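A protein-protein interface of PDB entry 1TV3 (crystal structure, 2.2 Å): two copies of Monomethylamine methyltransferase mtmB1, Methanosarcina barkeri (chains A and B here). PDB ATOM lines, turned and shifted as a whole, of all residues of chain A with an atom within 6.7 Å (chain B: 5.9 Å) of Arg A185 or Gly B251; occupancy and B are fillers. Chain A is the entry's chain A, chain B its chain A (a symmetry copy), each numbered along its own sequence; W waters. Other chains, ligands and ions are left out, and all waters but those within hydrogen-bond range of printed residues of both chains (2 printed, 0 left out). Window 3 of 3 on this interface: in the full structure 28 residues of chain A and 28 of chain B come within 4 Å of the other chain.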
ATOM      1  N   MET A 141     -32.134  18.476 -10.003  1.00  0.00           N
ATOM      2  CA  MET A 141     -33.536  18.532  -9.594  1.00  0.00           C
ATOM      3  C   MET A 141     -34.463  17.841 -10.593  1.00  0.00           C
ATOM      4  O   MET A 141     -35.312  17.040 -10.202  1.00  0.00           O
ATOM      5  CB  MET A 141     -33.977  19.982  -9.370  1.00  0.00           C
ATOM      6  CG  MET A 141     -33.443  20.582  -8.072  1.00  0.00           C
ATOM      7  SD  MET A 141     -34.111  22.232  -7.733  1.00  0.00           S
ATOM      8  CE  MET A 141     -35.830  21.836  -7.493  1.00  0.00           C
ATOM      9  N   VAL A 177     -18.997  18.964   2.240  1.00  0.00           N
ATOM     10  CA  VAL A 177     -19.987  19.408   3.219  1.00  0.00           C
ATOM     11  C   VAL A 177     -21.114  20.142   2.495  1.00  0.00           C
ATOM     12  O   VAL A 177     -22.290  19.895   2.757  1.00  0.00           O
ATOM     13  CB  VAL A 177     -19.350  20.355   4.276  1.00  0.00           C
ATOM     14  CG1 VAL A 177     -20.431  21.127   5.030  1.00  0.00           C
ATOM     15  CG2 VAL A 177     -18.522  19.539   5.256  1.00  0.00           C
ATOM     16  N   LEU A 178     -20.752  21.035   1.579  1.00  0.00           N
ATOM     17  CA  LEU A 178     -21.749  21.786   0.820  1.00  0.00           C
ATOM     18  C   LEU A 178     -22.686  20.842   0.065  1.00  0.00           C
ATOM     19  O   LEU A 178     -23.905  21.036   0.059  1.00  0.00           O
ATOM     20  CB  LEU A 178     -21.064  22.734  -0.172  1.00  0.00           C
ATOM     21  CG  LEU A 178     -21.987  23.542  -1.099  1.00  0.00           C
ATOM     22  CD1 LEU A 178     -22.939  24.420  -0.277  1.00  0.00           C
ATOM     23  CD2 LEU A 178     -21.140  24.406  -2.030  1.00  0.00           C
ATOM     24  N   ALA A 180     -23.293  17.642   0.763  1.00  0.00           N
ATOM     25  CA  ALA A 180     -24.072  16.826   1.695  1.00  0.00           C
ATOM     26  C   ALA A 180     -25.376  17.521   2.102  1.00  0.00           C
ATOM     27  O   ALA A 180     -26.432  16.889   2.175  1.00  0.00           O
ATOM     28  CB  ALA A 180     -23.238  16.505   2.937  1.00  0.00           C
ATOM     29  N   LYS A 181     -25.297  18.821   2.369  1.00  0.00           N
ATOM     30  CA  LYS A 181     -26.474  19.587   2.760  1.00  0.00           C
ATOM     31  C   LYS A 181     -27.341  19.898   1.541  1.00  0.00           C
ATOM     32  O   LYS A 181     -28.555  19.692   1.562  1.00  0.00           O
ATOM     33  CB  LYS A 181     -26.057  20.904   3.433  1.00  0.00           C
ATOM     34  CG  LYS A 181     -25.296  20.746   4.751  1.00  0.00           C
ATOM     35  CD  LYS A 181     -24.951  22.106   5.355  1.00  0.00           C
ATOM     36  CE  LYS A 181     -24.043  21.985   6.589  1.00  0.00           C
ATOM     37  NZ  LYS A 181     -24.682  21.269   7.744  1.00  0.00           N
ATOM     38  N   THR A 182     -26.697  20.388   0.483  1.00  0.00           N
ATOM     39  CA  THR A 182     -27.364  20.769  -0.758  1.00  0.00           C
ATOM     40  C   THR A 182     -28.136  19.632  -1.420  1.00  0.00           C
ATOM     41  O   THR A 182     -29.271  19.810  -1.870  1.00  0.00           O
ATOM     42  CB  THR A 182     -26.329  21.324  -1.763  1.00  0.00           C
ATOM     43  OG1 THR A 182     -25.690  22.472  -1.195  1.00  0.00           O
ATOM     44  CG2 THR A 182     -26.992  21.715  -3.069  1.00  0.00           C
ATOM     45  N   GLU A 183     -27.510  18.465  -1.476  1.00  0.00           N
ATOM     46  CA  GLU A 183     -28.111  17.287  -2.078  1.00  0.00           C
ATOM     47  C   GLU A 183     -29.600  17.138  -1.754  1.00  0.00           C
ATOM     48  O   GLU A 183     -30.452  17.247  -2.639  1.00  0.00           O
ATOM     49  CB  GLU A 183     -27.353  16.051  -1.605  1.00  0.00           C
ATOM     50  CG  GLU A 183     -27.849  14.734  -2.154  1.00  0.00           C
ATOM     51  CD  GLU A 183     -27.084  13.569  -1.557  1.00  0.00           C
ATOM     52  OE1 GLU A 183     -27.628  12.886  -0.662  1.00  0.00           O
ATOM     53  OE2 GLU A 183     -25.928  13.352  -1.974  1.00  0.00           O
ATOM     54  N   THR A 184     -29.911  16.890  -0.487  1.00  0.00           N
ATOM     55  CA  THR A 184     -31.300  16.707  -0.072  1.00  0.00           C
ATOM     56  C   THR A 184     -32.130  17.988  -0.170  1.00  0.00           C
ATOM     57  O   THR A 184     -33.336  17.933  -0.419  1.00  0.00           O
ATOM     58  CB  THR A 184     -31.366  16.126   1.361  1.00  0.00           C
ATOM     59  OG1 THR A 184     -30.803  14.807   1.353  1.00  0.00           O
ATOM     60  CG2 THR A 184     -32.807  16.041   1.857  1.00  0.00           C
ATOM     61  N   ARG A 185     -31.495  19.141   0.016  1.00  0.00           N
ATOM     62  CA  ARG A 185     -32.231  20.393  -0.097  1.00  0.00           C
ATOM     63  C   ARG A 185     -32.805  20.521  -1.505  1.00  0.00           C
ATOM     64  O   ARG A 185     -33.972  20.874  -1.675  1.00  0.00           O
ATOM     65  CB  ARG A 185     -31.322  21.581   0.221  1.00  0.00           C
ATOM     66  CG  ARG A 185     -31.172  21.827   1.711  1.00  0.00           C
ATOM     67  CD  ARG A 185     -30.132  22.883   2.024  1.00  0.00           C
ATOM     68  NE  ARG A 185     -30.204  23.281   3.427  1.00  0.00           N
ATOM     69  CZ  ARG A 185     -29.241  23.925   4.080  1.00  0.00           C
ATOM     70  NH1 ARG A 185     -28.111  24.248   3.464  1.00  0.00           N
ATOM     71  NH2 ARG A 185     -29.415  24.252   5.356  1.00  0.00           N
ATOM     72  N   LEU A 186     -31.989  20.213  -2.512  1.00  0.00           N
ATOM     73  CA  LEU A 186     -32.430  20.290  -3.905  1.00  0.00           C
ATOM     74  C   LEU A 186     -33.462  19.215  -4.226  1.00  0.00           C
ATOM     75  O   LEU A 186     -34.455  19.478  -4.903  1.00  0.00           O
ATOM     76  CB  LEU A 186     -31.241  20.130  -4.855  1.00  0.00           C
ATOM     77  CG  LEU A 186     -30.195  21.244  -4.840  1.00  0.00           C
ATOM     78  CD1 LEU A 186     -29.061  20.886  -5.794  1.00  0.00           C
ATOM     79  CD2 LEU A 186     -30.843  22.558  -5.239  1.00  0.00           C
ATOM     80  N   ILE A 187     -33.218  18.003  -3.738  1.00  0.00           N
ATOM     81  CA  ILE A 187     -34.125  16.895  -3.989  1.00  0.00           C
ATOM     82  C   ILE A 187     -35.505  17.137  -3.385  1.00  0.00           C
ATOM     83  O   ILE A 187     -36.521  16.878  -4.027  1.00  0.00           O
ATOM     84  CB  ILE A 187     -33.532  15.577  -3.460  1.00  0.00           C
ATOM     85  CG1 ILE A 187     -32.338  15.178  -4.337  1.00  0.00           C
ATOM     86  CG2 ILE A 187     -34.593  14.473  -3.458  1.00  0.00           C
ATOM     87  CD1 ILE A 187     -31.557  13.980  -3.833  1.00  0.00           C
ATOM     88  N   LYS A 188     -35.551  17.639  -2.157  1.00  0.00           N
ATOM     89  CA  LYS A 188     -36.838  17.905  -1.533  1.00  0.00           C
ATOM     90  C   LYS A 188     -37.540  19.038  -2.275  1.00  0.00           C
ATOM     91  O   LYS A 188     -38.770  19.101  -2.321  1.00  0.00           O
ATOM     92  CB  LYS A 188     -36.658  18.223  -0.044  1.00  0.00           C
ATOM     93  CG  LYS A 188     -36.354  16.964   0.769  1.00  0.00           C
ATOM     94  CD  LYS A 188     -36.386  17.185   2.278  1.00  0.00           C
ATOM     95  CE  LYS A 188     -36.228  15.848   3.009  1.00  0.00           C
ATOM     96  NZ  LYS A 188     -36.190  15.976   4.495  1.00  0.00           N
ATOM     97  N   ASN A 189     -36.751  19.918  -2.881  1.00  0.00           N
ATOM     98  CA  ASN A 189     -37.314  21.018  -3.648  1.00  0.00           C
ATOM     99  C   ASN A 189     -37.910  20.449  -4.931  1.00  0.00           C
ATOM    100  O   ASN A 189     -38.932  20.932  -5.425  1.00  0.00           O
ATOM    101  CB  ASN A 189     -36.236  22.034  -4.002  1.00  0.00           C
ATOM    102  CG  ASN A 189     -36.703  23.447  -3.796  1.00  0.00           C
ATOM    103  OD1 ASN A 189     -36.335  24.349  -4.547  1.00  0.00           O
ATOM    104  ND2 ASN A 189     -37.501  23.660  -2.752  1.00  0.00           N
ATOM    105  N   ALA A 190     -37.263  19.424  -5.476  1.00  0.00           N
ATOM    106  CA  ALA A 190     -37.766  18.786  -6.685  1.00  0.00           C
ATOM    107  C   ALA A 190     -39.084  18.095  -6.335  1.00  0.00           C
ATOM    108  O   ALA A 190     -40.033  18.112  -7.120  1.00  0.00           O
ATOM    109  CB  ALA A 190     -36.754  17.766  -7.206  1.00  0.00           C
ATOM    110  N   CYS A 218     -29.751  19.020   8.234  1.00  0.00           N
ATOM    111  CA  CYS A 218     -29.849  20.472   8.258  1.00  0.00           C
ATOM    112  C   CYS A 218     -31.247  20.942   7.874  1.00  0.00           C
ATOM    113  O   CYS A 218     -32.041  20.181   7.319  1.00  0.00           O
ATOM    114  CB  CYS A 218     -28.823  21.078   7.294  1.00  0.00           C
ATOM    115  SG  CYS A 218     -29.063  20.596   5.555  1.00  0.00           S
ATOM    116  N   THR A 219     -31.543  22.203   8.174  1.00  0.00           N
ATOM    117  CA  THR A 219     -32.843  22.775   7.852  1.00  0.00           C
ATOM    118  C   THR A 219     -33.036  22.758   6.342  1.00  0.00           C
ATOM    119  O   THR A 219     -32.171  23.216   5.594  1.00  0.00           O
ATOM    120  CB  THR A 219     -32.944  24.224   8.355  1.00  0.00           C
ATOM    121  OG1 THR A 219     -32.702  24.247   9.765  1.00  0.00           O
ATOM    122  CG2 THR A 219     -34.333  24.799   8.079  1.00  0.00           C
ATOM    123  N   GLY A 220     -34.166  22.219   5.898  1.00  0.00           N
ATOM    124  CA  GLY A 220     -34.446  22.146   4.475  1.00  0.00           C
ATOM    125  C   GLY A 220     -33.852  20.893   3.862  1.00  0.00           C
ATOM    126  O   GLY A 220     -34.210  20.506   2.747  1.00  0.00           O
ATOM    127  N   GLY A 221     -32.942  20.256   4.594  1.00  0.00           N
ATOM    128  CA  GLY A 221     -32.307  19.046   4.100  1.00  0.00           C
ATOM    129  C   GLY A 221     -32.781  17.792   4.813  1.00  0.00           C
ATOM    130  O   GLY A 221     -33.975  17.636   5.088  1.00  0.00           O
ATOM    131  N   MET A 222     -31.851  16.890   5.115  1.00  0.00           N
ATOM    132  CA  MET A 222     -32.206  15.654   5.796  1.00  0.00           C
ATOM    133  C   MET A 222     -32.670  15.919   7.222  1.00  0.00           C
ATOM    134  O   MET A 222     -32.115  16.770   7.912  1.00  0.00           O
ATOM    135  CB  MET A 222     -31.017  14.689   5.804  1.00  0.00           C
ATOM    136  CG  MET A 222     -30.628  14.198   4.420  1.00  0.00           C
ATOM    137  SD  MET A 222     -29.573  12.738   4.479  1.00  0.00           S
ATOM    138  CE  MET A 222     -30.770  11.488   5.027  1.00  0.00           C
ATOM    139  N   ILE B 246     -16.066  25.393   8.793  1.00  0.00           N
ATOM    140  CA  ILE B 246     -16.604  26.695   8.421  1.00  0.00           C
ATOM    141  C   ILE B 246     -17.749  26.524   7.409  1.00  0.00           C
ATOM    142  O   ILE B 246     -18.795  27.165   7.528  1.00  0.00           O
ATOM    143  CB  ILE B 246     -15.493  27.597   7.814  1.00  0.00           C
ATOM    144  CG1 ILE B 246     -14.500  27.996   8.912  1.00  0.00           C
ATOM    145  CG2 ILE B 246     -16.107  28.846   7.175  1.00  0.00           C
ATOM    146  CD1 ILE B 246     -13.208  28.606   8.393  1.00  0.00           C
ATOM    147  N   ALA B 247     -17.551  25.651   6.422  1.00  0.00           N
ATOM    148  CA  ALA B 247     -18.570  25.404   5.407  1.00  0.00           C
ATOM    149  C   ALA B 247     -19.856  24.898   6.057  1.00  0.00           C
ATOM    150  O   ALA B 247     -20.959  25.233   5.630  1.00  0.00           O
ATOM    151  CB  ALA B 247     -18.063  24.387   4.381  1.00  0.00           C
ATOM    152  N   HIS B 248     -19.706  24.086   7.095  1.00  0.00           N
ATOM    153  CA  HIS B 248     -20.849  23.539   7.809  1.00  0.00           C
ATOM    154  C   HIS B 248     -21.599  24.634   8.567  1.00  0.00           C
ATOM    155  O   HIS B 248     -22.823  24.724   8.485  1.00  0.00           O
ATOM    156  CB  HIS B 248     -20.370  22.442   8.761  1.00  0.00           C
ATOM    157  CG  HIS B 248     -21.371  22.060   9.805  1.00  0.00           C
ATOM    158  ND1 HIS B 248     -21.241  22.426  11.127  1.00  0.00           N
ATOM    159  CD2 HIS B 248     -22.508  21.329   9.725  1.00  0.00           C
ATOM    160  CE1 HIS B 248     -22.253  21.936  11.818  1.00  0.00           C
ATOM    161  NE2 HIS B 248     -23.037  21.267  10.991  1.00  0.00           N
ATOM    162  N   TYR B 249     -20.864  25.470   9.297  1.00  0.00           N
ATOM    163  CA  TYR B 249     -21.476  26.564  10.049  1.00  0.00           C
ATOM    164  C   TYR B 249     -22.274  27.476   9.119  1.00  0.00           C
ATOM    165  O   TYR B 249     -23.408  27.854   9.425  1.00  0.00           O
ATOM    166  CB  TYR B 249     -20.401  27.389  10.757  1.00  0.00           C
ATOM    167  CG  TYR B 249     -19.700  26.685  11.902  1.00  0.00           C
ATOM    168  CD1 TYR B 249     -18.496  27.181  12.406  1.00  0.00           C
ATOM    169  CD2 TYR B 249     -20.241  25.541  12.492  1.00  0.00           C
ATOM    170  CE1 TYR B 249     -17.845  26.559  13.467  1.00  0.00           C
ATOM    171  CE2 TYR B 249     -19.596  24.907  13.559  1.00  0.00           C
ATOM    172  CZ  TYR B 249     -18.398  25.426  14.040  1.00  0.00           C
ATOM    173  OH  TYR B 249     -17.746  24.818  15.092  1.00  0.00           O
ATOM    174  N   LYS B 250     -21.672  27.835   7.989  1.00  0.00           N
ATOM    175  CA  LYS B 250     -22.318  28.701   7.005  1.00  0.00           C
ATOM    176  C   LYS B 250     -23.584  28.035   6.467  1.00  0.00           C
ATOM    177  O   LYS B 250     -24.615  28.691   6.297  1.00  0.00           O
ATOM    178  CB  LYS B 250     -21.356  28.996   5.838  1.00  0.00           C
ATOM    179  CG  LYS B 250     -20.149  29.879   6.211  1.00  0.00           C
ATOM    180  CD  LYS B 250     -19.059  29.885   5.123  1.00  0.00           C
ATOM    181  CE  LYS B 250     -19.519  30.528   3.809  1.00  0.00           C
ATOM    182  NZ  LYS B 250     -19.861  31.976   3.964  1.00  0.00           N
ATOM    183  N   GLY B 251     -23.494  26.730   6.216  1.00  0.00           N
ATOM    184  CA  GLY B 251     -24.620  25.982   5.680  1.00  0.00           C
ATOM    185  C   GLY B 251     -25.802  25.820   6.617  1.00  0.00           C
ATOM    186  O   GLY B 251     -26.895  25.456   6.175  1.00  0.00           O
ATOM    187  N   ASN B 252     -25.587  26.084   7.905  1.00  0.00           N
ATOM    188  CA  ASN B 252     -26.641  25.974   8.912  1.00  0.00           C
ATOM    189  C   ASN B 252     -27.058  27.355   9.428  1.00  0.00           C
ATOM    190  O   ASN B 252     -27.825  27.460  10.385  1.00  0.00           O
ATOM    191  CB  ASN B 252     -26.162  25.122  10.099  1.00  0.00           C
ATOM    192  CG  ASN B 252     -26.212  23.623   9.818  1.00  0.00           C
ATOM    193  OD1 ASN B 252     -26.438  23.186   8.686  1.00  0.00           O
ATOM    194  ND2 ASN B 252     -25.989  22.825  10.861  1.00  0.00           N
ATOM    195  N   SER B 253     -26.539  28.408   8.804  1.00  0.00           N
ATOM    196  CA  SER B 253     -26.855  29.777   9.209  1.00  0.00           C
ATOM    197  C   SER B 253     -26.474  30.029  10.679  1.00  0.00           C
ATOM    198  O   SER B 253     -27.178  30.743  11.396  1.00  0.00           O
ATOM    199  CB  SER B 253     -28.355  30.050   8.997  1.00  0.00           C
ATOM    200  OG  SER B 253     -28.637  31.441   8.904  1.00  0.00           O
ATOM    201  N   ASP B 254     -25.356  29.445  11.115  1.00  0.00           N
ATOM    202  CA  ASP B 254     -24.869  29.599  12.490  1.00  0.00           C
ATOM    203  C   ASP B 254     -24.022  30.852  12.703  1.00  0.00           C
ATOM    204  O   ASP B 254     -23.282  31.271  11.809  1.00  0.00           O
ATOM    205  CB  ASP B 254     -23.981  28.415  12.896  1.00  0.00           C
ATOM    206  CG  ASP B 254     -24.741  27.123  13.044  1.00  0.00           C
ATOM    207  OD1 ASP B 254     -25.919  27.158  13.462  1.00  0.00           O
ATOM    208  OD2 ASP B 254     -24.137  26.066  12.768  1.00  0.00           O
HETATM  209  O   HOH W   1     -29.469  23.900   9.125  1.00  0.00           O
HETATM  210  O   HOH W   2     -25.759  19.997  10.607  1.00  0.00           O
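NZ of Lys A181 lies within hydrogen-bond range of OD1 of Asn B252, at 2.8 Å. NH2 of Arg A185 sits at hydrogen-bond distance from O of Gly B251, at 2.9 Å.
The guanidinium group of Arg A185 sits at hydrogen-bond distance from the side-chain sulfur of Cys A218 (3.6 Å). The guanidinium group of Arg A185 lies within hydrogen-bond range of the backbone carbonyl oxygen of Thr A219, at 2.9 Å. ND2 of Asn B252 is in hydrogen-bond range of NE2 of His B248.
Among the printed residues, pairs that only touch across the chains: Lys A181 with His B248, Cys A218 with Asn B252, Val A177 with His B248, Lys A181 with Gly B251 and Val A177 with Ala B247.
Of the printed residues of chain B, Val A177 touches Ala B247 and His B248. Of the printed residues of chain B, Lys A181 touches His B248 (2.9 Å), Gly B251 (3.9 Å) and Asn B252 (2.8 Å). Of chain B, only Gly B251 comes within 4 Å of Arg A185. Leu A186 touches none of the printed residues of chain B. Tyr B249 touches none of the printed residues of chain A. Gly B251 touches two residues of chain A. Of the printed residues of chain A, Asn B252 touches Lys A181 (2.8 Å) and Cys A218 (3.5 Å). The nearest residue of chain A that does not touch Gly B251 is Cys A218 (4.9 Å).
Of the 9 printed residues of chain B, 4 touch a printed residue of chain A. Of the 19 printed residues of chain A, 4 touch a printed residue of chain B. Printed residues of chain A that touch a printed residue of chain B: Val A177, Lys A181, Arg A185 and Cys A218. Hydrophobic or aromatic side chains of chain A that line the printed part of chain B: Val A177. Among the printed residues, 7 pairs touch across the chains. Among the printed residues, no Asp or Glu carboxylate lies within 4 Å of a Lys or Arg side-chain nitrogen of the other chain.
No position is printed for both chains.
Water W1 lies within hydrogen-bond range of N of Thr A219 (2.8 Å) and OD1 of Asn B252 (3.1 Å). Water W2 lies within hydrogen-bond range of ND2 of Asn B252 (2.8 Å), NE2 of His B248 (3.0 Å) and NZ of Lys A181 (3.3 Å).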
